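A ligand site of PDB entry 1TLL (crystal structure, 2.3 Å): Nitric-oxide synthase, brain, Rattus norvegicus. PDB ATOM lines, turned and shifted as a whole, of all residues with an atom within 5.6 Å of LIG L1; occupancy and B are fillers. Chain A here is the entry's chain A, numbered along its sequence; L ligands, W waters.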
ATOM      1  N   ALA A  19      22.875  24.921  -1.107  1.00  0.00           N
ATOM      2  CA  ALA A  19      23.360  24.497  -2.420  1.00  0.00           C
ATOM      3  C   ALA A  19      22.839  25.632  -3.273  1.00  0.00           C
ATOM      4  O   ALA A  19      21.760  26.149  -3.021  1.00  0.00           O
ATOM      5  CB  ALA A  19      22.713  23.171  -2.832  1.00  0.00           C
ATOM      6  N   THR A  20      23.602  26.045  -4.278  1.00  0.00           N
ATOM      7  CA  THR A  20      23.201  27.172  -5.095  1.00  0.00           C
ATOM      8  C   THR A  20      23.977  27.097  -6.414  1.00  0.00           C
ATOM      9  O   THR A  20      24.957  26.355  -6.517  1.00  0.00           O
ATOM     10  CB  THR A  20      23.530  28.487  -4.316  1.00  0.00           C
ATOM     11  OG1 THR A  20      23.125  29.634  -5.064  1.00  0.00           O
ATOM     12  CG2 THR A  20      25.029  28.566  -4.040  1.00  0.00           C
ATOM     13  N   GLU A  21      23.523  27.828  -7.428  1.00  0.00           N
ATOM     14  CA  GLU A  21      24.204  27.841  -8.719  1.00  0.00           C
ATOM     15  C   GLU A  21      24.490  29.277  -9.125  1.00  0.00           C
ATOM     16  O   GLU A  21      25.401  29.531  -9.909  1.00  0.00           O
ATOM     17  CB  GLU A  21      23.359  27.171  -9.805  1.00  0.00           C
ATOM     18  CG  GLU A  21      23.446  25.653  -9.843  1.00  0.00           C
ATOM     19  CD  GLU A  21      24.736  25.133 -10.463  1.00  0.00           C
ATOM     20  OE1 GLU A  21      25.160  25.685 -11.506  1.00  0.00           O
ATOM     21  OE2 GLU A  21      25.322  24.161  -9.931  1.00  0.00           O
ATOM     22  N   THR A  22      23.710  30.219  -8.603  1.00  0.00           N
ATOM     23  CA  THR A  22      23.934  31.627  -8.930  1.00  0.00           C
ATOM     24  C   THR A  22      24.071  32.476  -7.668  1.00  0.00           C
ATOM     25  O   THR A  22      24.235  33.695  -7.756  1.00  0.00           O
ATOM     26  CB  THR A  22      22.805  32.198  -9.815  1.00  0.00           C
ATOM     27  OG1 THR A  22      21.606  32.369  -9.055  1.00  0.00           O
ATOM     28  CG2 THR A  22      22.516  31.248 -10.975  1.00  0.00           C
ATOM     29  N   GLY A  23      24.003  31.844  -6.500  1.00  0.00           N
ATOM     30  CA  GLY A  23      24.183  32.566  -5.252  1.00  0.00           C
ATOM     31  C   GLY A  23      22.993  32.957  -4.390  1.00  0.00           C
ATOM     32  O   GLY A  23      23.182  33.440  -3.275  1.00  0.00           O
ATOM     33  N   LYS A  24      21.772  32.760  -4.870  1.00  0.00           N
ATOM     34  CA  LYS A  24      20.602  33.115  -4.087  1.00  0.00           C
ATOM     35  C   LYS A  24      20.458  32.272  -2.824  1.00  0.00           C
ATOM     36  O   LYS A  24      20.266  32.800  -1.731  1.00  0.00           O
ATOM     37  CB  LYS A  24      19.342  33.021  -4.923  1.00  0.00           C
ATOM     38  CG  LYS A  24      19.204  34.138  -5.945  1.00  0.00           C
ATOM     39  CD  LYS A  24      17.850  34.093  -6.620  1.00  0.00           C
ATOM     40  CE  LYS A  24      17.985  33.763  -8.097  1.00  0.00           C
ATOM     41  NZ  LYS A  24      16.693  33.318  -8.700  1.00  0.00           N
ATOM     42  N   SER A  25      20.527  30.954  -2.953  1.00  0.00           N
ATOM     43  CA  SER A  25      20.372  30.124  -1.759  1.00  0.00           C
ATOM     44  C   SER A  25      21.429  30.515  -0.743  1.00  0.00           C
ATOM     45  O   SER A  25      21.154  30.600   0.450  1.00  0.00           O
ATOM     46  CB  SER A  25      20.489  28.649  -2.106  1.00  0.00           C
ATOM     47  OG  SER A  25      19.489  28.285  -3.036  1.00  0.00           O
ATOM     48  N   GLN A  26      22.641  30.768  -1.217  1.00  0.00           N
ATOM     49  CA  GLN A  26      23.752  31.128  -0.354  1.00  0.00           C
ATOM     50  C   GLN A  26      23.460  32.409   0.428  1.00  0.00           C
ATOM     51  O   GLN A  26      23.752  32.482   1.618  1.00  0.00           O
ATOM     52  CB  GLN A  26      25.002  31.305  -1.185  1.00  0.00           C
ATOM     53  CG  GLN A  26      26.220  31.658  -0.380  1.00  0.00           C
ATOM     54  CD  GLN A  26      27.367  31.986  -1.282  1.00  0.00           C
ATOM     55  OE1 GLN A  26      27.303  32.968  -2.020  1.00  0.00           O
ATOM     56  NE2 GLN A  26      28.423  31.173  -1.239  1.00  0.00           N
ATOM     57  N   SER A  66      18.476  25.438  -4.137  1.00  0.00           N
ATOM     58  CA  SER A  66      17.765  25.655  -5.382  1.00  0.00           C
ATOM     59  C   SER A  66      17.756  24.312  -6.103  1.00  0.00           C
ATOM     60  O   SER A  66      18.183  23.302  -5.568  1.00  0.00           O
ATOM     61  CB  SER A  66      18.469  26.703  -6.233  1.00  0.00           C
ATOM     62  OG  SER A  66      19.817  26.332  -6.450  1.00  0.00           O
ATOM     63  N   THR A  67      17.239  24.313  -7.322  1.00  0.00           N
ATOM     64  CA  THR A  67      17.175  23.114  -8.130  1.00  0.00           C
ATOM     65  C   THR A  67      17.687  23.601  -9.452  1.00  0.00           C
ATOM     66  O   THR A  67      17.456  24.752  -9.806  1.00  0.00           O
ATOM     67  CB  THR A  67      15.723  22.631  -8.332  1.00  0.00           C
ATOM     68  OG1 THR A  67      15.142  22.316  -7.062  1.00  0.00           O
ATOM     69  CG2 THR A  67      15.673  21.381  -9.180  1.00  0.00           C
ATOM     70  N   PHE A  68      18.398  22.755 -10.178  1.00  0.00           N
ATOM     71  CA  PHE A  68      18.894  23.175 -11.468  1.00  0.00           C
ATOM     72  C   PHE A  68      18.697  22.152 -12.552  1.00  0.00           C
ATOM     73  O   PHE A  68      18.117  21.089 -12.341  1.00  0.00           O
ATOM     74  CB  PHE A  68      20.361  23.586 -11.366  1.00  0.00           C
ATOM     75  CG  PHE A  68      20.579  25.033 -11.664  1.00  0.00           C
ATOM     76  CD1 PHE A  68      20.279  26.014 -10.704  1.00  0.00           C
ATOM     77  CD2 PHE A  68      21.003  25.428 -12.922  1.00  0.00           C
ATOM     78  CE1 PHE A  68      20.401  27.368 -11.008  1.00  0.00           C
ATOM     79  CE2 PHE A  68      21.129  26.769 -13.228  1.00  0.00           C
ATOM     80  CZ  PHE A  68      20.828  27.750 -12.268  1.00  0.00           C
ATOM     81  N   GLY A  69      19.156  22.512 -13.750  1.00  0.00           N
ATOM     82  CA  GLY A  69      19.024  21.626 -14.885  1.00  0.00           C
ATOM     83  C   GLY A  69      17.619  21.095 -15.013  1.00  0.00           C
ATOM     84  O   GLY A  69      16.644  21.838 -14.974  1.00  0.00           O
ATOM     85  N   ASN A  70      17.522  19.772 -15.123  1.00  0.00           N
ATOM     86  CA  ASN A  70      16.236  19.115 -15.277  1.00  0.00           C
ATOM     87  C   ASN A  70      15.731  18.526 -13.956  1.00  0.00           C
ATOM     88  O   ASN A  70      15.595  17.314 -13.810  1.00  0.00           O
ATOM     89  CB  ASN A  70      16.387  18.016 -16.339  1.00  0.00           C
ATOM     90  CG  ASN A  70      15.056  17.570 -16.892  1.00  0.00           C
ATOM     91  OD1 ASN A  70      14.099  18.334 -16.917  1.00  0.00           O
ATOM     92  ND2 ASN A  70      15.016  16.320 -17.381  1.00  0.00           N
ATOM     93  N   GLY A  71      15.437  19.405 -12.996  1.00  0.00           N
ATOM     94  CA  GLY A  71      14.957  18.960 -11.695  1.00  0.00           C
ATOM     95  C   GLY A  71      16.094  18.350 -10.893  1.00  0.00           C
ATOM     96  O   GLY A  71      15.885  17.520 -10.031  1.00  0.00           O
ATOM     97  N   ASP A  72      17.315  18.802 -11.171  1.00  0.00           N
ATOM     98  CA  ASP A  72      18.478  18.239 -10.501  1.00  0.00           C
ATOM     99  C   ASP A  72      19.083  19.081  -9.372  1.00  0.00           C
ATOM    100  O   ASP A  72      18.700  20.233  -9.157  1.00  0.00           O
ATOM    101  CB  ASP A  72      19.555  17.944 -11.541  1.00  0.00           C
ATOM    102  CG  ASP A  72      19.083  16.934 -12.569  1.00  0.00           C
ATOM    103  OD1 ASP A  72      19.156  17.240 -13.782  1.00  0.00           O
ATOM    104  OD2 ASP A  72      18.635  15.830 -12.159  1.00  0.00           O
ATOM    105  N   PRO A  74      21.837  21.311  -7.313  1.00  0.00           N
ATOM    106  CA  PRO A  74      22.740  22.293  -7.910  1.00  0.00           C
ATOM    107  C   PRO A  74      24.006  21.458  -7.987  1.00  0.00           C
ATOM    108  O   PRO A  74      24.094  20.405  -7.334  1.00  0.00           O
ATOM    109  CB  PRO A  74      22.839  23.380  -6.850  1.00  0.00           C
ATOM    110  CG  PRO A  74      21.500  23.313  -6.205  1.00  0.00           C
ATOM    111  CD  PRO A  74      21.224  21.843  -6.081  1.00  0.00           C
ATOM    112  N   LEU A 143      14.408  26.831  -3.450  1.00  0.00           N
ATOM    113  CA  LEU A 143      14.254  27.859  -4.446  1.00  0.00           C
ATOM    114  C   LEU A 143      13.994  27.132  -5.772  1.00  0.00           C
ATOM    115  O   LEU A 143      14.468  25.995  -5.969  1.00  0.00           O
ATOM    116  CB  LEU A 143      15.530  28.681  -4.554  1.00  0.00           C
ATOM    117  CG  LEU A 143      15.921  29.599  -3.394  1.00  0.00           C
ATOM    118  CD1 LEU A 143      16.246  28.788  -2.164  1.00  0.00           C
ATOM    119  CD2 LEU A 143      17.133  30.414  -3.807  1.00  0.00           C
ATOM    120  N   GLY A 144      13.249  27.782  -6.669  1.00  0.00           N
ATOM    121  CA  GLY A 144      12.923  27.178  -7.947  1.00  0.00           C
ATOM    122  C   GLY A 144      12.135  28.119  -8.836  1.00  0.00           C
ATOM    123  O   GLY A 144      12.205  29.329  -8.665  1.00  0.00           O
ATOM    124  N   SER A 145      11.417  27.572  -9.806  1.00  0.00           N
ATOM    125  CA  SER A 145      10.609  28.383 -10.711  1.00  0.00           C
ATOM    126  C   SER A 145       9.445  27.576 -11.263  1.00  0.00           C
ATOM    127  O   SER A 145       9.614  26.418 -11.667  1.00  0.00           O
ATOM    128  CB  SER A 145      11.457  28.905 -11.866  1.00  0.00           C
ATOM    129  OG  SER A 145      10.631  29.513 -12.840  1.00  0.00           O
ATOM    130  N   ARG A 146       8.253  28.176 -11.270  1.00  0.00           N
ATOM    131  CA  ARG A 146       7.064  27.486 -11.758  1.00  0.00           C
ATOM    132  C   ARG A 146       7.160  27.295 -13.250  1.00  0.00           C
ATOM    133  O   ARG A 146       6.322  26.614 -13.848  1.00  0.00           O
ATOM    134  CB  ARG A 146       5.800  28.294 -11.466  1.00  0.00           C
ATOM    135  CG  ARG A 146       5.469  28.431 -10.006  1.00  0.00           C
ATOM    136  CD  ARG A 146       4.853  27.202  -9.396  1.00  0.00           C
ATOM    137  NE  ARG A 146       4.459  27.504  -8.032  1.00  0.00           N
ATOM    138  CZ  ARG A 146       3.834  26.653  -7.222  1.00  0.00           C
ATOM    139  NH1 ARG A 146       3.531  25.434  -7.657  1.00  0.00           N
ATOM    140  NH2 ARG A 146       3.529  27.026  -5.981  1.00  0.00           N
ATOM    141  N   TYR A 148       9.331  25.661 -14.616  1.00  0.00           N
ATOM    142  CA  TYR A 148       9.891  24.335 -14.823  1.00  0.00           C
ATOM    143  C   TYR A 148       8.974  23.227 -14.307  1.00  0.00           C
ATOM    144  O   TYR A 148       8.261  23.392 -13.306  1.00  0.00           O
ATOM    145  CB  TYR A 148      11.248  24.229 -14.118  1.00  0.00           C
ATOM    146  CG  TYR A 148      12.306  25.151 -14.712  1.00  0.00           C
ATOM    147  CD1 TYR A 148      13.251  24.668 -15.619  1.00  0.00           C
ATOM    148  CD2 TYR A 148      12.327  26.523 -14.411  1.00  0.00           C
ATOM    149  CE1 TYR A 148      14.189  25.519 -16.213  1.00  0.00           C
ATOM    150  CE2 TYR A 148      13.265  27.374 -15.004  1.00  0.00           C
ATOM    151  CZ  TYR A 148      14.182  26.874 -15.894  1.00  0.00           C
ATOM    152  OH  TYR A 148      15.108  27.755 -16.407  1.00  0.00           O
ATOM    153  N   HIS A 150       9.472  20.174 -12.771  1.00  0.00           N
ATOM    154  CA  HIS A 150       9.682  19.705 -11.405  1.00  0.00           C
ATOM    155  C   HIS A 150      10.117  20.849 -10.515  1.00  0.00           C
ATOM    156  O   HIS A 150      11.303  21.000 -10.215  1.00  0.00           O
ATOM    157  CB  HIS A 150      10.711  18.578 -11.450  1.00  0.00           C
ATOM    158  CG  HIS A 150      10.457  17.609 -12.556  1.00  0.00           C
ATOM    159  ND1 HIS A 150       9.347  16.799 -12.588  1.00  0.00           N
ATOM    160  CD2 HIS A 150      11.112  17.399 -13.736  1.00  0.00           C
ATOM    161  CE1 HIS A 150       9.317  16.141 -13.725  1.00  0.00           C
ATOM    162  NE2 HIS A 150      10.367  16.485 -14.442  1.00  0.00           N
ATOM    163  N   PHE A 151       9.144  21.641 -10.108  1.00  0.00           N
ATOM    164  CA  PHE A 151       9.327  22.810  -9.269  1.00  0.00           C
ATOM    165  C   PHE A 151       9.959  22.455  -7.925  1.00  0.00           C
ATOM    166  O   PHE A 151       9.418  21.650  -7.180  1.00  0.00           O
ATOM    167  CB  PHE A 151       7.959  23.488  -9.052  1.00  0.00           C
ATOM    168  CG  PHE A 151       8.020  24.769  -8.259  1.00  0.00           C
ATOM    169  CD1 PHE A 151       8.936  25.763  -8.582  1.00  0.00           C
ATOM    170  CD2 PHE A 151       7.122  24.987  -7.209  1.00  0.00           C
ATOM    171  CE1 PHE A 151       8.983  26.956  -7.871  1.00  0.00           C
ATOM    172  CE2 PHE A 151       7.157  26.182  -6.491  1.00  0.00           C
ATOM    173  CZ  PHE A 151       8.081  27.165  -6.826  1.00  0.00           C
ATOM    174  N   CYS A 152      11.124  23.053  -7.635  1.00  0.00           N
ATOM    175  CA  CYS A 152      11.835  22.804  -6.376  1.00  0.00           C
ATOM    176  C   CYS A 152      12.091  21.334  -6.078  1.00  0.00           C
ATOM    177  O   CYS A 152      12.029  20.908  -4.935  1.00  0.00           O
ATOM    178  CB  CYS A 152      11.061  23.425  -5.199  1.00  0.00           C
ATOM    179  SG  CYS A 152      10.806  25.209  -5.352  1.00  0.00           S
ATOM    180  N   ALA A 153      12.432  20.574  -7.112  1.00  0.00           N
ATOM    181  CA  ALA A 153      12.661  19.138  -6.961  1.00  0.00           C
ATOM    182  C   ALA A 153      13.730  18.726  -5.951  1.00  0.00           C
ATOM    183  O   ALA A 153      13.516  17.807  -5.156  1.00  0.00           O
ATOM    184  CB  ALA A 153      12.994  18.543  -8.312  1.00  0.00           C
ATOM    185  N   GLU A 178      11.041  31.978  -8.035  1.00  0.00           N
ATOM    186  CA  GLU A 178      11.819  33.066  -8.635  1.00  0.00           C
ATOM    187  C   GLU A 178      10.940  33.987  -9.455  1.00  0.00           C
ATOM    188  O   GLU A 178      11.271  35.146  -9.688  1.00  0.00           O
ATOM    189  CB  GLU A 178      12.901  32.474  -9.547  1.00  0.00           C
ATOM    190  CG  GLU A 178      13.965  33.476  -9.952  1.00  0.00           C
ATOM    191  CD  GLU A 178      14.523  33.208 -11.341  1.00  0.00           C
ATOM    192  OE1 GLU A 178      14.772  32.028 -11.684  1.00  0.00           O
ATOM    193  OE2 GLU A 178      14.716  34.194 -12.072  1.00  0.00           O
ATOM    194  N   GLN A 182       9.996  35.370  -4.316  1.00  0.00           N
ATOM    195  CA  GLN A 182      10.976  34.425  -3.772  1.00  0.00           C
ATOM    196  C   GLN A 182      11.583  34.942  -2.478  1.00  0.00           C
ATOM    197  O   GLN A 182      11.488  34.292  -1.447  1.00  0.00           O
ATOM    198  CB  GLN A 182      12.095  34.152  -4.778  1.00  0.00           C
ATOM    199  CG  GLN A 182      12.974  32.977  -4.387  1.00  0.00           C
ATOM    200  CD  GLN A 182      13.968  32.593  -5.482  1.00  0.00           C
ATOM    201  OE1 GLN A 182      14.971  33.278  -5.691  1.00  0.00           O
ATOM    202  NE2 GLN A 182      13.678  31.495  -6.191  1.00  0.00           N
ATOM    203  N   ILE A 653      18.621  21.028 -20.591  1.00  0.00           N
ATOM    204  CA  ILE A 653      17.833  22.257 -20.411  1.00  0.00           C
ATOM    205  C   ILE A 653      18.607  23.558 -20.330  1.00  0.00           C
ATOM    206  O   ILE A 653      19.442  23.749 -19.444  1.00  0.00           O
ATOM    207  CB  ILE A 653      16.949  22.137 -19.129  1.00  0.00           C
ATOM    208  CG1 ILE A 653      16.187  20.808 -19.135  1.00  0.00           C
ATOM    209  CG2 ILE A 653      15.992  23.317 -19.041  1.00  0.00           C
ATOM    210  CD1 ILE A 653      15.299  20.622 -20.340  1.00  0.00           C
ATOM    211  N   PHE A 654      18.303  24.460 -21.251  1.00  0.00           N
ATOM    212  CA  PHE A 654      18.932  25.774 -21.292  1.00  0.00           C
ATOM    213  C   PHE A 654      18.226  26.731 -20.337  1.00  0.00           C
ATOM    214  O   PHE A 654      18.720  27.825 -20.066  1.00  0.00           O
ATOM    215  CB  PHE A 654      18.841  26.392 -22.695  1.00  0.00           C
ATOM    216  CG  PHE A 654      19.767  25.784 -23.707  1.00  0.00           C
ATOM    217  CD1 PHE A 654      19.930  26.406 -24.938  1.00  0.00           C
ATOM    218  CD2 PHE A 654      20.442  24.600 -23.456  1.00  0.00           C
ATOM    219  CE1 PHE A 654      20.753  25.851 -25.891  1.00  0.00           C
ATOM    220  CE2 PHE A 654      21.269  24.048 -24.418  1.00  0.00           C
ATOM    221  CZ  PHE A 654      21.424  24.681 -25.639  1.00  0.00           C
ATOM    222  N   GLY A 655      17.070  26.313 -19.837  1.00  0.00           N
ATOM    223  CA  GLY A 655      16.323  27.195 -18.962  1.00  0.00           C
ATOM    224  C   GLY A 655      15.221  27.826 -19.799  1.00  0.00           C
ATOM    225  O   GLY A 655      14.846  27.274 -20.841  1.00  0.00           O
HETATM  226  N1  LIG L   1      13.711  25.577 -10.700  1.00  0.00           N
HETATM  227  C1  LIG L   1      12.894  24.584 -10.336  1.00  0.00           C
HETATM  228  O1  LIG L   1      11.975  24.563  -9.487  1.00  0.00           O
HETATM  229  N2  LIG L   1      13.107  23.317 -11.058  1.00  0.00           N
HETATM  230  C2  LIG L   1      14.123  23.105 -12.125  1.00  0.00           C
HETATM  231  O2  LIG L   1      14.093  21.937 -12.590  1.00  0.00           O
HETATM  232  C3  LIG L   1      14.889  24.153 -12.441  1.00  0.00           C
HETATM  233  N3  LIG L   1      15.789  24.064 -13.402  1.00  0.00           N
HETATM  234  C4  LIG L   1      16.641  25.212 -13.847  1.00  0.00           C
HETATM  235  C5  LIG L   1      17.575  25.138 -14.957  1.00  0.00           C
HETATM  236  C6  LIG L   1      18.352  26.349 -15.373  1.00  0.00           C
HETATM  237  C7  LIG L   1      19.177  25.984 -16.522  1.00  0.00           C
HETATM  238  C8  LIG L   1      18.197  27.684 -14.654  1.00  0.00           C
HETATM  239  C9  LIG L   1      18.938  28.927 -15.043  1.00  0.00           C
HETATM  240  C10 LIG L   1      17.314  27.748 -13.581  1.00  0.00           C
HETATM  241  C11 LIG L   1      16.450  26.519 -13.106  1.00  0.00           C
HETATM  242  N4  LIG L   1      15.497  26.676 -11.994  1.00  0.00           N
HETATM  243  C12 LIG L   1      14.676  25.515 -11.661  1.00  0.00           C
HETATM  244  C13 LIG L   1      15.299  27.888 -11.278  1.00  0.00           C
HETATM  245  C14 LIG L   1      16.298  28.000 -10.124  1.00  0.00           C
HETATM  246  O3  LIG L   1      16.087  26.946  -9.306  1.00  0.00           O
HETATM  247  C15 LIG L   1      16.005  29.252  -9.515  1.00  0.00           C
HETATM  248  O4  LIG L   1      16.309  30.358 -10.525  1.00  0.00           O
HETATM  249  C16 LIG L   1      16.799  29.653  -8.294  1.00  0.00           C
HETATM  250  O5  LIG L   1      16.329  30.912  -7.889  1.00  0.00           O
HETATM  251  C17 LIG L   1      18.353  29.772  -8.484  1.00  0.00           C
HETATM  252  O6  LIG L   1      18.807  29.637  -7.169  1.00  0.00           O
HETATM  253  P1  LIG L   1      20.335  29.655  -6.873  1.00  0.00           P
HETATM  254  O7  LIG L   1      20.486  29.499  -5.476  1.00  0.00           O
HETATM  255  O8  LIG L   1      21.016  28.448  -7.501  1.00  0.00           O
HETATM  256  O9  LIG L   1      20.761  31.005  -7.232  1.00  0.00           O
HETATM  257  P1  LG2 L   2      21.727  37.588 -19.265  1.00  0.00           P
HETATM  258  O1  LG2 L   2      22.042  38.936 -19.227  1.00  0.00           O
HETATM  259  O2  LG2 L   2      21.952  36.940 -18.192  1.00  0.00           O
HETATM  260  O3  LG2 L   2      20.143  37.832 -19.475  1.00  0.00           O
HETATM  261  C1  LG2 L   2      19.069  36.886 -19.625  1.00  0.00           C
HETATM  262  C2  LG2 L   2      17.854  37.331 -18.616  1.00  0.00           C
HETATM  263  O4  LG2 L   2      17.157  38.303 -19.493  1.00  0.00           O
HETATM  264  C3  LG2 L   2      16.830  36.452 -18.441  1.00  0.00           C
HETATM  265  O5  LG2 L   2      17.042  35.695 -17.356  1.00  0.00           O
HETATM  266  C4  LG2 L   2      15.588  37.244 -18.377  1.00  0.00           C
HETATM  267  O6  LG2 L   2      15.216  37.581 -17.062  1.00  0.00           O
HETATM  268  C5  LG2 L   2      15.770  38.367 -19.046  1.00  0.00           C
HETATM  269  N1  LG2 L   2      15.613  38.761 -20.630  1.00  0.00           N
HETATM  270  C6  LG2 L   2      15.708  38.005 -21.940  1.00  0.00           C
HETATM  271  N2  LG2 L   2      14.881  38.159 -22.783  1.00  0.00           N
HETATM  272  C7  LG2 L   2      14.053  39.002 -22.283  1.00  0.00           C
HETATM  273  C8  LG2 L   2      12.749  39.614 -22.897  1.00  0.00           C
HETATM  274  N3  LG2 L   2      12.304  39.262 -24.206  1.00  0.00           N
HETATM  275  N4  LG2 L   2      12.046  40.480 -22.196  1.00  0.00           N
HETATM  276  C9  LG2 L   2      12.385  40.972 -20.773  1.00  0.00           C
HETATM  277  N5  LG2 L   2      13.597  40.462 -20.061  1.00  0.00           N
HETATM  278  C10 LG2 L   2      14.388  39.458 -20.937  1.00  0.00           C
HETATM  279  N6  LG2 L   2      22.621  29.718 -25.043  1.00  0.00           N
HETATM  280  C11 LG2 L   2      23.078  29.710 -26.320  1.00  0.00           C
HETATM  281  O7  LG2 L   2      22.945  30.586 -27.068  1.00  0.00           O
HETATM  282  N7  LG2 L   2      23.720  28.592 -26.754  1.00  0.00           N
HETATM  283  C12 LG2 L   2      23.927  27.458 -25.907  1.00  0.00           C
HETATM  284  O8  LG2 L   2      24.479  26.590 -26.349  1.00  0.00           O
HETATM  285  C13 LG2 L   2      23.439  27.483 -24.604  1.00  0.00           C
HETATM  286  N8  LG2 L   2      23.682  26.324 -23.826  1.00  0.00           N
HETATM  287  C14 LG2 L   2      23.243  26.280 -22.510  1.00  0.00           C
HETATM  288  C15 LG2 L   2      23.472  25.169 -21.792  1.00  0.00           C
HETATM  289  C16 LG2 L   2      23.097  25.069 -20.485  1.00  0.00           C
HETATM  290  C17 LG2 L   2      23.433  23.771 -19.859  1.00  0.00           C
HETATM  291  C18 LG2 L   2      22.359  26.300 -19.764  1.00  0.00           C
HETATM  292  C19 LG2 L   2      21.971  26.257 -18.404  1.00  0.00           C
HETATM  293  C20 LG2 L   2      22.078  27.453 -20.404  1.00  0.00           C
HETATM  294  C21 LG2 L   2      22.500  27.522 -21.832  1.00  0.00           C
HETATM  295  N9  LG2 L   2      22.334  28.612 -22.762  1.00  0.00           N
HETATM  296  C22 LG2 L   2      22.793  28.620 -24.157  1.00  0.00           C
HETATM  297  C23 LG2 L   2      21.639  29.946 -22.286  1.00  0.00           C
HETATM  298  C24 LG2 L   2      22.938  30.901 -21.887  1.00  0.00           C
HETATM  299  O9  LG2 L   2      23.797  30.376 -21.023  1.00  0.00           O
HETATM  300  C25 LG2 L   2      22.636  32.431 -21.391  1.00  0.00           C
HETATM  301  O10 LG2 L   2      21.492  32.227 -20.468  1.00  0.00           O
HETATM  302  C26 LG2 L   2      22.212  33.298 -22.414  1.00  0.00           C
HETATM  303  O11 LG2 L   2      23.322  33.489 -23.531  1.00  0.00           O
HETATM  304  C27 LG2 L   2      21.884  34.679 -21.909  1.00  0.00           C
HETATM  305  O12 LG2 L   2      22.852  35.089 -21.225  1.00  0.00           O
HETATM  306  P2  LG2 L   2      23.289  36.634 -21.354  1.00  0.00           P
HETATM  307  O13 LG2 L   2      24.284  36.360 -20.473  1.00  0.00           O
HETATM  308  O14 LG2 L   2      23.505  37.085 -22.518  1.00  0.00           O
HETATM  309  O15 LG2 L   2      21.918  37.580 -20.707  1.00  0.00           O
HETATM  310  O   HOH W   1      12.067  20.792 -14.263  1.00  0.00           O
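The side-chain carboxylate (OE1) of Glu 178 lies within salt-bridge range of the side-chain amino group (NZ) of Lys 24 (3.8 Å). OG1 of Thr 20 is in hydrogen-bond range of N of Gly 23, at 2.8 Å. The backbone NH (N) of Ala 153 is in hydrogen-bond range of the side-chain hydroxyl (OG1) of Thr 67 (3.2 Å). O of Leu 143 sits close to SG of Cys 152 (3.8 Å). The side-chain hydroxyl (OG) of Ser 25 lies close to the backbone carbonyl oxygen (O) of Ala 19, 3.1 Å away. The side-chain amide oxygen (OE1) of Gln 182 lies close to the side-chain amino group (NZ) of Lys 24 (3.5 Å). N of Glu 178 lies close to NE2 of Gln 182 (3.3 Å). The backbone NH of Ser 66 sits at hydrogen-bond distance from the side-chain hydroxyl of Ser 25 (3.2 Å).
The backbone carbonyl oxygen of Gly 69 sits close to a nitrogen (N3) of LIG L1, at 2.9 Å. Phe 68 touches LIG L1. O of Leu 143 touches O3 of LIG L1, 3.8 Å away. Gly 144 touches LIG L1 (CA to O1, 3.2 Å). Tyr 148 touches LIG L1 (CE1 to C4, 3.4 Å). Phe 151 touches LIG L1 (CA to O1, 3.2 Å). O of Ile 653 touches C7 of LIG L1, at 3.7 Å. Gly 655 touches LIG L1 (N to C7, 3.9 Å). Hydrophobic or aromatic side chains within 4 Å of LIG L1: Phe 68, Leu 143, Tyr 148 and Phe 151. 22 residues have an atom within 4 Å of LIG L1: Thr 20, Glu 21, Thr 22, Gly 23, Lys 24, Ser 25, Ser 66, Thr 67, Phe 68, Gly 69, Gly 71, Leu 143, Gly 144, Ser 145, Tyr 148, His 150, Phe 151, Cys 152, Glu 178, Gln 182, Ile 653 and Gly 655.
Water W1 lies within hydrogen-bond range of O2 of LIG L1 and N of His 150.
NZ of Lys 24 is in hydrogen-bond range of O5 of LIG L1 (2.6 Å). O3 of LIG L1 is in hydrogen-bond range of O of Thr 67 (2.6 Å). The backbone NH of Lys 24 lies within hydrogen-bond range of an oxygen (O9) of LIG L1 (3.1 Å). O1 of LIG L1 is in hydrogen-bond range of N of Cys 152. N of Thr 22 sits at hydrogen-bond distance from O9 of LIG L1 (3.3 Å). O4 of LIG L1 is in hydrogen-bond range of OE1 of Glu 178 (2.5 Å). The backbone NH (N) of Ser 145 lies within hydrogen-bond range of an oxygen (O1) of LIG L1, at 3.1 Å. The side-chain hydroxyl (OG) of Ser 25 lies within hydrogen-bond range of an oxygen (O7) of LIG L1 (2.9 Å). The side-chain hydroxyl (OG) of Ser 66 sits at hydrogen-bond distance from an oxygen (O8) of LIG L1, 2.6 Å away. The side-chain hydroxyl of Thr 22 sits at hydrogen-bond distance from an oxygen (O9) of LIG L1 (2.4 Å). The backbone NH (N) of Ser 25 lies within hydrogen-bond range of an oxygen (O7) of LIG L1, 2.9 Å away. NE2 of Gln 182 lies within hydrogen-bond range of O5 of LIG L1 (3.2 Å). O7 of LIG L1 lies within hydrogen-bond range of OG1 of Thr 20. N of Thr 67 lies within hydrogen-bond range of O3 of LIG L1 (3.5 Å). The backbone NH (N) of Glu 21 is in hydrogen-bond range of an oxygen (O8) of LIG L1, at 2.6 Å. An oxygen (O2) of LIG L1 is in hydrogen-bond range of the backbone NH of Gly 71. N2 of LIG L1 lies within hydrogen-bond range of O of His 150, 3.1 Å away. An oxygen (O9) of LIG L1 sits at hydrogen-bond distance from the backbone NH (N) of Gly 23, at 3.4 Å.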
